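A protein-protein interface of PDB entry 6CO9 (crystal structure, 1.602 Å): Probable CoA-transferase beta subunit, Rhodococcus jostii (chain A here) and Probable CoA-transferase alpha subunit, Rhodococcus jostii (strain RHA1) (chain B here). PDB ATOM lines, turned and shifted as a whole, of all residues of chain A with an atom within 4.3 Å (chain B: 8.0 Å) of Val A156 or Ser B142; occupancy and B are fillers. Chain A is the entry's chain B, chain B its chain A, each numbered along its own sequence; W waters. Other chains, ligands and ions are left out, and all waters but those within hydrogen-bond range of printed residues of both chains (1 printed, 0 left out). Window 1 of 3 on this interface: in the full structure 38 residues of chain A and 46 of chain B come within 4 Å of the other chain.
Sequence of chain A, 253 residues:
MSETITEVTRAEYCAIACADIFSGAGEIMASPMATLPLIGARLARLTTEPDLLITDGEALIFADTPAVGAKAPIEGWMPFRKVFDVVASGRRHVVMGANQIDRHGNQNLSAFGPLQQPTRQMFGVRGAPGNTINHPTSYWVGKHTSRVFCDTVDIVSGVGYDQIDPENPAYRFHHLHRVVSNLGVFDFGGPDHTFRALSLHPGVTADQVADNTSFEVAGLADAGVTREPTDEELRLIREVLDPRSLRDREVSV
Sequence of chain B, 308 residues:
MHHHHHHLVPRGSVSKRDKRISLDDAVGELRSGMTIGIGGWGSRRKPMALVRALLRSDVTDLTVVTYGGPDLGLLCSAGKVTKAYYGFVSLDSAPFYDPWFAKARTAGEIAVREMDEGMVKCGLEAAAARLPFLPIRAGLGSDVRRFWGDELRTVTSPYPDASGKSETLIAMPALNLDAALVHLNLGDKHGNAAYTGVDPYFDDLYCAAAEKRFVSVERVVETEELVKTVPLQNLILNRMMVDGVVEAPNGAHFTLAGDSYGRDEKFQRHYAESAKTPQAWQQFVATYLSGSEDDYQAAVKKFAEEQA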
ATOM      1  N   ASN A 106     -17.256 -13.971  25.997  1.00  0.00           N
ATOM      2  CA  ASN A 106     -17.677 -12.898  25.114  1.00  0.00           C
ATOM      3  C   ASN A 106     -17.555 -13.377  23.679  1.00  0.00           C
ATOM      4  O   ASN A 106     -16.610 -14.089  23.329  1.00  0.00           O
ATOM      5  CB  ASN A 106     -16.840 -11.638  25.309  1.00  0.00           C
ATOM      6  CG  ASN A 106     -16.892 -11.133  26.724  1.00  0.00           C
ATOM      7  OD1 ASN A 106     -15.914 -11.238  27.471  1.00  0.00           O
ATOM      8  ND2 ASN A 106     -18.056 -10.644  27.126  1.00  0.00           N
ATOM      9  N   GLN A 107     -18.511 -12.986  22.853  1.00  0.00           N
ATOM     10  CA  GLN A 107     -18.596 -13.488  21.489  1.00  0.00           C
ATOM     11  C   GLN A 107     -18.835 -12.329  20.527  1.00  0.00           C
ATOM     12  O   GLN A 107     -19.452 -11.320  20.890  1.00  0.00           O
ATOM     13  CB  GLN A 107     -19.710 -14.569  21.410  1.00  0.00           C
ATOM     14  CG  GLN A 107     -20.012 -15.115  20.015  1.00  0.00           C
ATOM     15  CD  GLN A 107     -21.159 -14.395  19.316  1.00  0.00           C
ATOM     16  OE1 GLN A 107     -21.512 -13.283  19.673  1.00  0.00           O
ATOM     17  NE2 GLN A 107     -21.736 -15.030  18.306  1.00  0.00           N
ATOM     18  N   PRO A 129     -27.069 -10.163  21.594  1.00  0.00           N
ATOM     19  CA  PRO A 129     -27.198  -9.578  22.944  1.00  0.00           C
ATOM     20  C   PRO A 129     -28.439 -10.078  23.670  1.00  0.00           C
ATOM     21  O   PRO A 129     -28.364 -10.485  24.840  1.00  0.00           O
ATOM     22  CB  PRO A 129     -27.235  -8.065  22.664  1.00  0.00           C
ATOM     23  CG  PRO A 129     -26.548  -7.887  21.309  1.00  0.00           C
ATOM     24  CD  PRO A 129     -26.932  -9.125  20.541  1.00  0.00           C
ATOM     25  N   VAL A 153     -12.312 -10.094  22.166  1.00  0.00           N
ATOM     26  CA  VAL A 153     -13.125  -9.950  20.963  1.00  0.00           C
ATOM     27  C   VAL A 153     -13.197  -8.478  20.583  1.00  0.00           C
ATOM     28  O   VAL A 153     -13.093  -7.585  21.436  1.00  0.00           O
ATOM     29  CB  VAL A 153     -14.533 -10.564  21.138  1.00  0.00           C
ATOM     30  CG1 VAL A 153     -14.435 -12.001  21.659  1.00  0.00           C
ATOM     31  CG2 VAL A 153     -15.425  -9.711  22.044  1.00  0.00           C
ATOM     32  N   ILE A 155     -15.774  -6.797  19.140  1.00  0.00           N
ATOM     33  CA  ILE A 155     -17.090  -6.244  19.440  1.00  0.00           C
ATOM     34  C   ILE A 155     -17.848  -7.305  20.221  1.00  0.00           C
ATOM     35  O   ILE A 155     -17.923  -8.456  19.779  1.00  0.00           O
ATOM     36  CB  ILE A 155     -17.856  -5.865  18.154  1.00  0.00           C
ATOM     37  CG1 ILE A 155     -17.068  -4.830  17.345  1.00  0.00           C
ATOM     38  CG2 ILE A 155     -19.258  -5.359  18.480  1.00  0.00           C
ATOM     39  CD1 ILE A 155     -17.699  -4.510  16.004  1.00  0.00           C
ATOM     40  N   VAL A 156     -18.374  -6.939  21.391  1.00  0.00           N
ATOM     41  CA  VAL A 156     -19.115  -7.892  22.222  1.00  0.00           C
ATOM     42  C   VAL A 156     -20.563  -7.916  21.737  1.00  0.00           C
ATOM     43  O   VAL A 156     -21.363  -7.052  22.098  1.00  0.00           O
ATOM     44  CB  VAL A 156     -19.021  -7.547  23.711  1.00  0.00           C
ATOM     45  CG1 VAL A 156     -19.862  -8.513  24.547  1.00  0.00           C
ATOM     46  CG2 VAL A 156     -17.563  -7.552  24.167  1.00  0.00           C
ATOM     47  N   SER A 157     -20.903  -8.896  20.895  1.00  0.00           N
ATOM     48  CA  SER A 157     -22.297  -9.114  20.519  1.00  0.00           C
ATOM     49  C   SER A 157     -22.957 -10.131  21.439  1.00  0.00           C
ATOM     50  O   SER A 157     -24.145  -9.998  21.749  1.00  0.00           O
ATOM     51  CB  SER A 157     -22.418  -9.553  19.051  1.00  0.00           C
ATOM     52  OG  SER A 157     -21.622 -10.681  18.741  1.00  0.00           O
ATOM     53  N   GLY A 158     -22.214 -11.151  21.860  1.00  0.00           N
ATOM     54  CA  GLY A 158     -22.685 -12.116  22.840  1.00  0.00           C
ATOM     55  C   GLY A 158     -22.002 -11.866  24.178  1.00  0.00           C
ATOM     56  O   GLY A 158     -20.776 -11.761  24.250  1.00  0.00           O
ATOM     57  N   VAL A 159     -22.816 -11.793  25.227  1.00  0.00           N
ATOM     58  CA  VAL A 159     -22.356 -11.366  26.547  1.00  0.00           C
ATOM     59  C   VAL A 159     -21.626 -12.509  27.245  1.00  0.00           C
ATOM     60  O   VAL A 159     -22.164 -13.616  27.370  1.00  0.00           O
ATOM     61  CB  VAL A 159     -23.549 -10.882  27.392  1.00  0.00           C
ATOM     62  CG1 VAL A 159     -23.090 -10.446  28.775  1.00  0.00           C
ATOM     63  CG2 VAL A 159     -24.286  -9.752  26.685  1.00  0.00           C
ATOM     64  N   GLN A 163     -18.994  -9.668  32.114  1.00  0.00           N
ATOM     65  CA  GLN A 163     -19.864  -8.507  31.977  1.00  0.00           C
ATOM     66  C   GLN A 163     -20.964  -8.461  33.025  1.00  0.00           C
ATOM     67  O   GLN A 163     -21.679  -7.456  33.107  1.00  0.00           O
ATOM     68  CB  GLN A 163     -20.525  -8.490  30.596  1.00  0.00           C
ATOM     69  CG  GLN A 163     -19.588  -8.766  29.439  1.00  0.00           C
ATOM     70  CD  GLN A 163     -18.581  -7.665  29.228  1.00  0.00           C
ATOM     71  OE1 GLN A 163     -18.653  -6.602  29.852  1.00  0.00           O
ATOM     72  NE2 GLN A 163     -17.630  -7.908  28.338  1.00  0.00           N
ATOM     73  N   GLU B 114     -26.151   0.517  15.882  1.00  0.00           N
ATOM     74  CA  GLU B 114     -26.399  -0.912  15.869  1.00  0.00           C
ATOM     75  C   GLU B 114     -26.992  -1.362  17.206  1.00  0.00           C
ATOM     76  O   GLU B 114     -26.643  -0.845  18.271  1.00  0.00           O
ATOM     77  CB  GLU B 114     -25.069  -1.610  15.571  1.00  0.00           C
ATOM     78  CG  GLU B 114     -25.128  -3.092  15.400  1.00  0.00           C
ATOM     79  CD  GLU B 114     -23.820  -3.632  14.859  1.00  0.00           C
ATOM     80  OE1 GLU B 114     -23.281  -3.052  13.891  1.00  0.00           O
ATOM     81  OE2 GLU B 114     -23.321  -4.625  15.413  1.00  0.00           O
ATOM     82  N   MET B 115     -27.926  -2.311  17.155  1.00  0.00           N
ATOM     83  CA  MET B 115     -28.621  -2.724  18.368  1.00  0.00           C
ATOM     84  C   MET B 115     -29.081  -4.165  18.211  1.00  0.00           C
ATOM     85  O   MET B 115     -29.080  -4.722  17.112  1.00  0.00           O
ATOM     86  CB  MET B 115     -29.811  -1.798  18.660  1.00  0.00           C
ATOM     87  CG  MET B 115     -30.971  -1.944  17.669  1.00  0.00           C
ATOM     88  SD  MET B 115     -32.278  -0.715  17.927  1.00  0.00           S
ATOM     89  CE  MET B 115     -31.919   0.426  16.594  1.00  0.00           C
ATOM     90  N   ASP B 116     -29.473  -4.773  19.329  1.00  0.00           N
ATOM     91  CA  ASP B 116     -30.065  -6.104  19.279  1.00  0.00           C
ATOM     92  C   ASP B 116     -31.363  -6.069  18.468  1.00  0.00           C
ATOM     93  O   ASP B 116     -32.086  -5.069  18.460  1.00  0.00           O
ATOM     94  CB  ASP B 116     -30.327  -6.606  20.697  1.00  0.00           C
ATOM     95  CG  ASP B 116     -31.036  -7.943  20.722  1.00  0.00           C
ATOM     96  OD1 ASP B 116     -30.352  -8.991  20.620  1.00  0.00           O
ATOM     97  OD2 ASP B 116     -32.283  -7.951  20.863  1.00  0.00           O
ATOM     98  N   MET B 119     -34.383  -5.019  20.191  1.00  0.00           N
ATOM     99  CA  MET B 119     -34.453  -3.601  20.514  1.00  0.00           C
ATOM    100  C   MET B 119     -35.114  -2.802  19.394  1.00  0.00           C
ATOM    101  O   MET B 119     -35.742  -1.769  19.668  1.00  0.00           O
ATOM    102  CB  MET B 119     -33.056  -3.042  20.798  1.00  0.00           C
ATOM    103  CG  MET B 119     -32.456  -3.489  22.130  1.00  0.00           C
ATOM    104  SD  MET B 119     -30.692  -3.101  22.289  1.00  0.00           S
ATOM    105  CE  MET B 119     -30.676  -1.330  22.361  1.00  0.00           C
ATOM    106  N   ARG B 137     -34.315  -6.089  28.415  1.00  0.00           N
ATOM    107  CA  ARG B 137     -33.078  -6.700  28.894  1.00  0.00           C
ATOM    108  C   ARG B 137     -31.990  -6.666  27.821  1.00  0.00           C
ATOM    109  O   ARG B 137     -30.835  -6.323  28.112  1.00  0.00           O
ATOM    110  CB  ARG B 137     -33.374  -8.138  29.328  1.00  0.00           C
ATOM    111  CG  ARG B 137     -32.291  -8.794  30.131  1.00  0.00           C
ATOM    112  CD  ARG B 137     -32.751 -10.149  30.672  1.00  0.00           C
ATOM    113  NE  ARG B 137     -34.205 -10.197  30.821  1.00  0.00           N
ATOM    114  CZ  ARG B 137     -34.825 -10.013  31.974  1.00  0.00           C
ATOM    115  NH1 ARG B 137     -34.106  -9.735  33.055  1.00  0.00           N
ATOM    116  NH2 ARG B 137     -36.153 -10.064  32.034  1.00  0.00           N
ATOM    117  N   ALA B 138     -32.354  -7.016  26.583  1.00  0.00           N
ATOM    118  CA  ALA B 138     -31.404  -7.069  25.477  1.00  0.00           C
ATOM    119  C   ALA B 138     -30.588  -5.785  25.375  1.00  0.00           C
ATOM    120  O   ALA B 138     -31.131  -4.676  25.402  1.00  0.00           O
ATOM    121  CB  ALA B 138     -32.149  -7.325  24.167  1.00  0.00           C
ATOM    122  N   GLY B 139     -29.280  -5.951  25.232  1.00  0.00           N
ATOM    123  CA  GLY B 139     -28.371  -4.823  25.177  1.00  0.00           C
ATOM    124  C   GLY B 139     -27.457  -4.770  26.383  1.00  0.00           C
ATOM    125  O   GLY B 139     -26.284  -4.391  26.270  1.00  0.00           O
ATOM    126  N   LEU B 140     -27.982  -5.141  27.548  1.00  0.00           N
ATOM    127  CA  LEU B 140     -27.189  -5.119  28.773  1.00  0.00           C
ATOM    128  C   LEU B 140     -25.943  -5.982  28.635  1.00  0.00           C
ATOM    129  O   LEU B 140     -26.010  -7.124  28.174  1.00  0.00           O
ATOM    130  CB  LEU B 140     -28.024  -5.627  29.948  1.00  0.00           C
ATOM    131  CG  LEU B 140     -29.049  -4.707  30.603  1.00  0.00           C
ATOM    132  CD1 LEU B 140     -29.841  -5.511  31.637  1.00  0.00           C
ATOM    133  CD2 LEU B 140     -28.358  -3.509  31.254  1.00  0.00           C
ATOM    134  N   GLY B 141     -24.804  -5.445  29.062  1.00  0.00           N
ATOM    135  CA  GLY B 141     -23.564  -6.200  29.061  1.00  0.00           C
ATOM    136  C   GLY B 141     -22.890  -6.357  27.716  1.00  0.00           C
ATOM    137  O   GLY B 141     -21.850  -7.024  27.643  1.00  0.00           O
ATOM    138  N   SER B 142     -23.443  -5.767  26.661  1.00  0.00           N
ATOM    139  CA  SER B 142     -22.924  -5.905  25.305  1.00  0.00           C
ATOM    140  C   SER B 142     -22.388  -4.583  24.788  1.00  0.00           C
ATOM    141  O   SER B 142     -22.614  -3.511  25.357  1.00  0.00           O
ATOM    142  CB  SER B 142     -24.012  -6.405  24.349  1.00  0.00           C
ATOM    143  OG  SER B 142     -24.894  -5.346  24.025  1.00  0.00           O
ATOM    144  N   ASP B 143     -21.705  -4.669  23.652  1.00  0.00           N
ATOM    145  CA  ASP B 143     -21.193  -3.439  23.070  1.00  0.00           C
ATOM    146  C   ASP B 143     -22.277  -2.615  22.389  1.00  0.00           C
ATOM    147  O   ASP B 143     -21.967  -1.554  21.846  1.00  0.00           O
ATOM    148  CB  ASP B 143     -20.051  -3.754  22.105  1.00  0.00           C
ATOM    149  CG  ASP B 143     -18.700  -3.718  22.786  1.00  0.00           C
ATOM    150  OD1 ASP B 143     -18.592  -3.040  23.831  1.00  0.00           O
ATOM    151  OD2 ASP B 143     -17.737  -4.340  22.283  1.00  0.00           O
ATOM    152  N   VAL B 144     -23.545  -3.031  22.440  1.00  0.00           N
ATOM    153  CA  VAL B 144     -24.604  -2.106  22.055  1.00  0.00           C
ATOM    154  C   VAL B 144     -24.479  -0.805  22.845  1.00  0.00           C
ATOM    155  O   VAL B 144     -24.695   0.289  22.306  1.00  0.00           O
ATOM    156  CB  VAL B 144     -25.988  -2.755  22.232  1.00  0.00           C
ATOM    157  CG1 VAL B 144     -27.070  -1.742  21.922  1.00  0.00           C
ATOM    158  CG2 VAL B 144     -26.116  -3.963  21.326  1.00  0.00           C
ATOM    159  N   ARG B 145     -24.071  -0.895  24.121  1.00  0.00           N
ATOM    160  CA  ARG B 145     -23.875   0.317  24.918  1.00  0.00           C
ATOM    161  C   ARG B 145     -22.826   1.233  24.299  1.00  0.00           C
ATOM    162  O   ARG B 145     -22.979   2.459  24.324  1.00  0.00           O
ATOM    163  CB  ARG B 145     -23.482  -0.031  26.356  1.00  0.00           C
ATOM    164  CG  ARG B 145     -24.463  -0.943  27.060  1.00  0.00           C
ATOM    165  CD  ARG B 145     -25.828  -0.300  27.217  1.00  0.00           C
ATOM    166  NE  ARG B 145     -25.820   0.996  27.890  1.00  0.00           N
ATOM    167  CZ  ARG B 145     -25.788   1.163  29.207  1.00  0.00           C
ATOM    168  NH1 ARG B 145     -25.733   0.109  30.012  1.00  0.00           N
ATOM    169  NH2 ARG B 145     -25.795   2.387  29.728  1.00  0.00           N
ATOM    170  N   ARG B 146     -21.758   0.654  23.725  1.00  0.00           N
ATOM    171  CA  ARG B 146     -20.672   1.442  23.144  1.00  0.00           C
ATOM    172  C   ARG B 146     -21.045   2.019  21.780  1.00  0.00           C
ATOM    173  O   ARG B 146     -20.554   3.094  21.414  1.00  0.00           O
ATOM    174  CB  ARG B 146     -19.413   0.575  23.040  1.00  0.00           C
ATOM    175  CG  ARG B 146     -18.127   1.334  22.742  1.00  0.00           C
ATOM    176  CD  ARG B 146     -16.935   0.734  23.490  1.00  0.00           C
ATOM    177  NE  ARG B 146     -16.625  -0.635  23.067  1.00  0.00           N
ATOM    178  CZ  ARG B 146     -15.840  -0.952  22.039  1.00  0.00           C
ATOM    179  NH1 ARG B 146     -15.280   0.004  21.309  1.00  0.00           N
ATOM    180  NH2 ARG B 146     -15.621  -2.230  21.737  1.00  0.00           N
ATOM    181  N   PHE B 147     -21.896   1.326  21.015  1.00  0.00           N
ATOM    182  CA  PHE B 147     -22.391   1.895  19.762  1.00  0.00           C
ATOM    183  C   PHE B 147     -23.182   3.175  20.011  1.00  0.00           C
ATOM    184  O   PHE B 147     -23.103   4.130  19.224  1.00  0.00           O
ATOM    185  CB  PHE B 147     -23.285   0.889  19.032  1.00  0.00           C
ATOM    186  CG  PHE B 147     -22.550  -0.138  18.218  1.00  0.00           C
ATOM    187  CD1 PHE B 147     -21.857   0.221  17.076  1.00  0.00           C
ATOM    188  CD2 PHE B 147     -22.606  -1.477  18.569  1.00  0.00           C
ATOM    189  CE1 PHE B 147     -21.215  -0.737  16.315  1.00  0.00           C
ATOM    190  CE2 PHE B 147     -21.971  -2.438  17.822  1.00  0.00           C
ATOM    191  CZ  PHE B 147     -21.269  -2.068  16.682  1.00  0.00           C
ATOM    192  N   LEU B 152     -28.128   5.943  24.686  1.00  0.00           N
ATOM    193  CA  LEU B 152     -28.824   4.786  25.248  1.00  0.00           C
ATOM    194  C   LEU B 152     -28.578   4.769  26.751  1.00  0.00           C
ATOM    195  O   LEU B 152     -27.441   4.577  27.199  1.00  0.00           O
ATOM    196  CB  LEU B 152     -28.351   3.486  24.598  1.00  0.00           C
ATOM    197  CG  LEU B 152     -29.137   2.223  24.937  1.00  0.00           C
ATOM    198  CD1 LEU B 152     -30.574   2.337  24.416  1.00  0.00           C
ATOM    199  CD2 LEU B 152     -28.432   1.015  24.348  1.00  0.00           C
ATOM    200  N   ILE B 170     -32.172  -1.741  30.099  1.00  0.00           N
ATOM    201  CA  ILE B 170     -32.024  -0.780  29.015  1.00  0.00           C
ATOM    202  C   ILE B 170     -33.332  -0.023  28.856  1.00  0.00           C
ATOM    203  O   ILE B 170     -34.415  -0.626  28.840  1.00  0.00           O
ATOM    204  CB  ILE B 170     -31.638  -1.481  27.701  1.00  0.00           C
ATOM    205  CG1 ILE B 170     -30.314  -2.240  27.852  1.00  0.00           C
ATOM    206  CG2 ILE B 170     -31.578  -0.468  26.544  1.00  0.00           C
ATOM    207  CD1 ILE B 170     -29.088  -1.338  27.978  1.00  0.00           C
HETATM  208  O   HOH W   1     -27.406  -8.012  25.980  1.00  0.00           O
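OD2 of Asp B143 lies within hydrogen-bond range of N of Val A156 (2.8 Å).
Of chain B, only Gly B141, Ser B142 and Asp B143 come within 4 Å of Val A156.
Ser B142 touches just these residues of chain A: Pro A129 and Val A156.
Of the printed residues of chain B, Gln A163 touches Gly B141.
Printed residues of chain A within 4 Å of Val B144: Pro A129.
Printed residues of chain A within 4 Å of Asp B143: Ile A155 (3.5 Å) and Val A156 (2.8 Å).
Met B115 touches none of the printed residues of chain A.
The nearest residue of chain B that does not touch Val A156 is Val B144 (4.6 Å).
The nearest residue of chain A that does not touch Ser B142 is Val A159 (4.1 Å).
The nearest printed residue of chain A that does not touch Gly B141 is Asn A106 (5.3 Å).
Water W1 lies within hydrogen-bond range of the backbone carbonyl oxygen (O) of Leu B140, the backbone NH (N) of Gly B139 and the backbone carbonyl oxygen (O) of Pro A129.
Of the 10 printed residues of chain A, 5 touch a printed residue of chain B.
Hydrophobic or aromatic side chains of chain B within 4 Å of the printed part of chain A: Val B144.
Among the printed residues, no Asp or Glu carboxylate lies within 4 Å of a Lys or Arg side-chain nitrogen of the other chain.
The side-chain sulfur (SD) of Met B119 is in hydrogen-bond range of the backbone NH (N) of Asp B116 (3.6 Å).
The side-chain hydroxyl of Ser B142 is in hydrogen-bond range of the backbone carbonyl oxygen of Gly B139 (2.8 Å).
OG of Ser B142 lies close to N of Val B144 (3.1 Å).
The guanidinium group (NH2) of Arg B146 is in salt-bridge range of the side-chain carboxylate (OD2) of Asp B143.
The side-chain amide nitrogen (ND2) of Asn A106 lies close to the side-chain amide nitrogen (NE2) of Gln A163, 3.0 Å away.
Among the printed residues, pairs that only touch across the chains: Gln A163 with Gly B141 (3.4 Å), Pro A129 with Asp B116 (3.4 Å), Val A159 with Leu B140 (3.5 Å), Ile A155 with Asp B143 (3.5 Å), Val A156 with Ser B142 (3.5 Å), Val A159 with Gly B141 (3.8 Å), Pro A129 with Ser B142 (3.8 Å), Pro A129 with Gly B139 (3.9 Å), Pro A129 with Val B144 (3.9 Å) and Val A156 with Gly B141 (3.97 Å).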
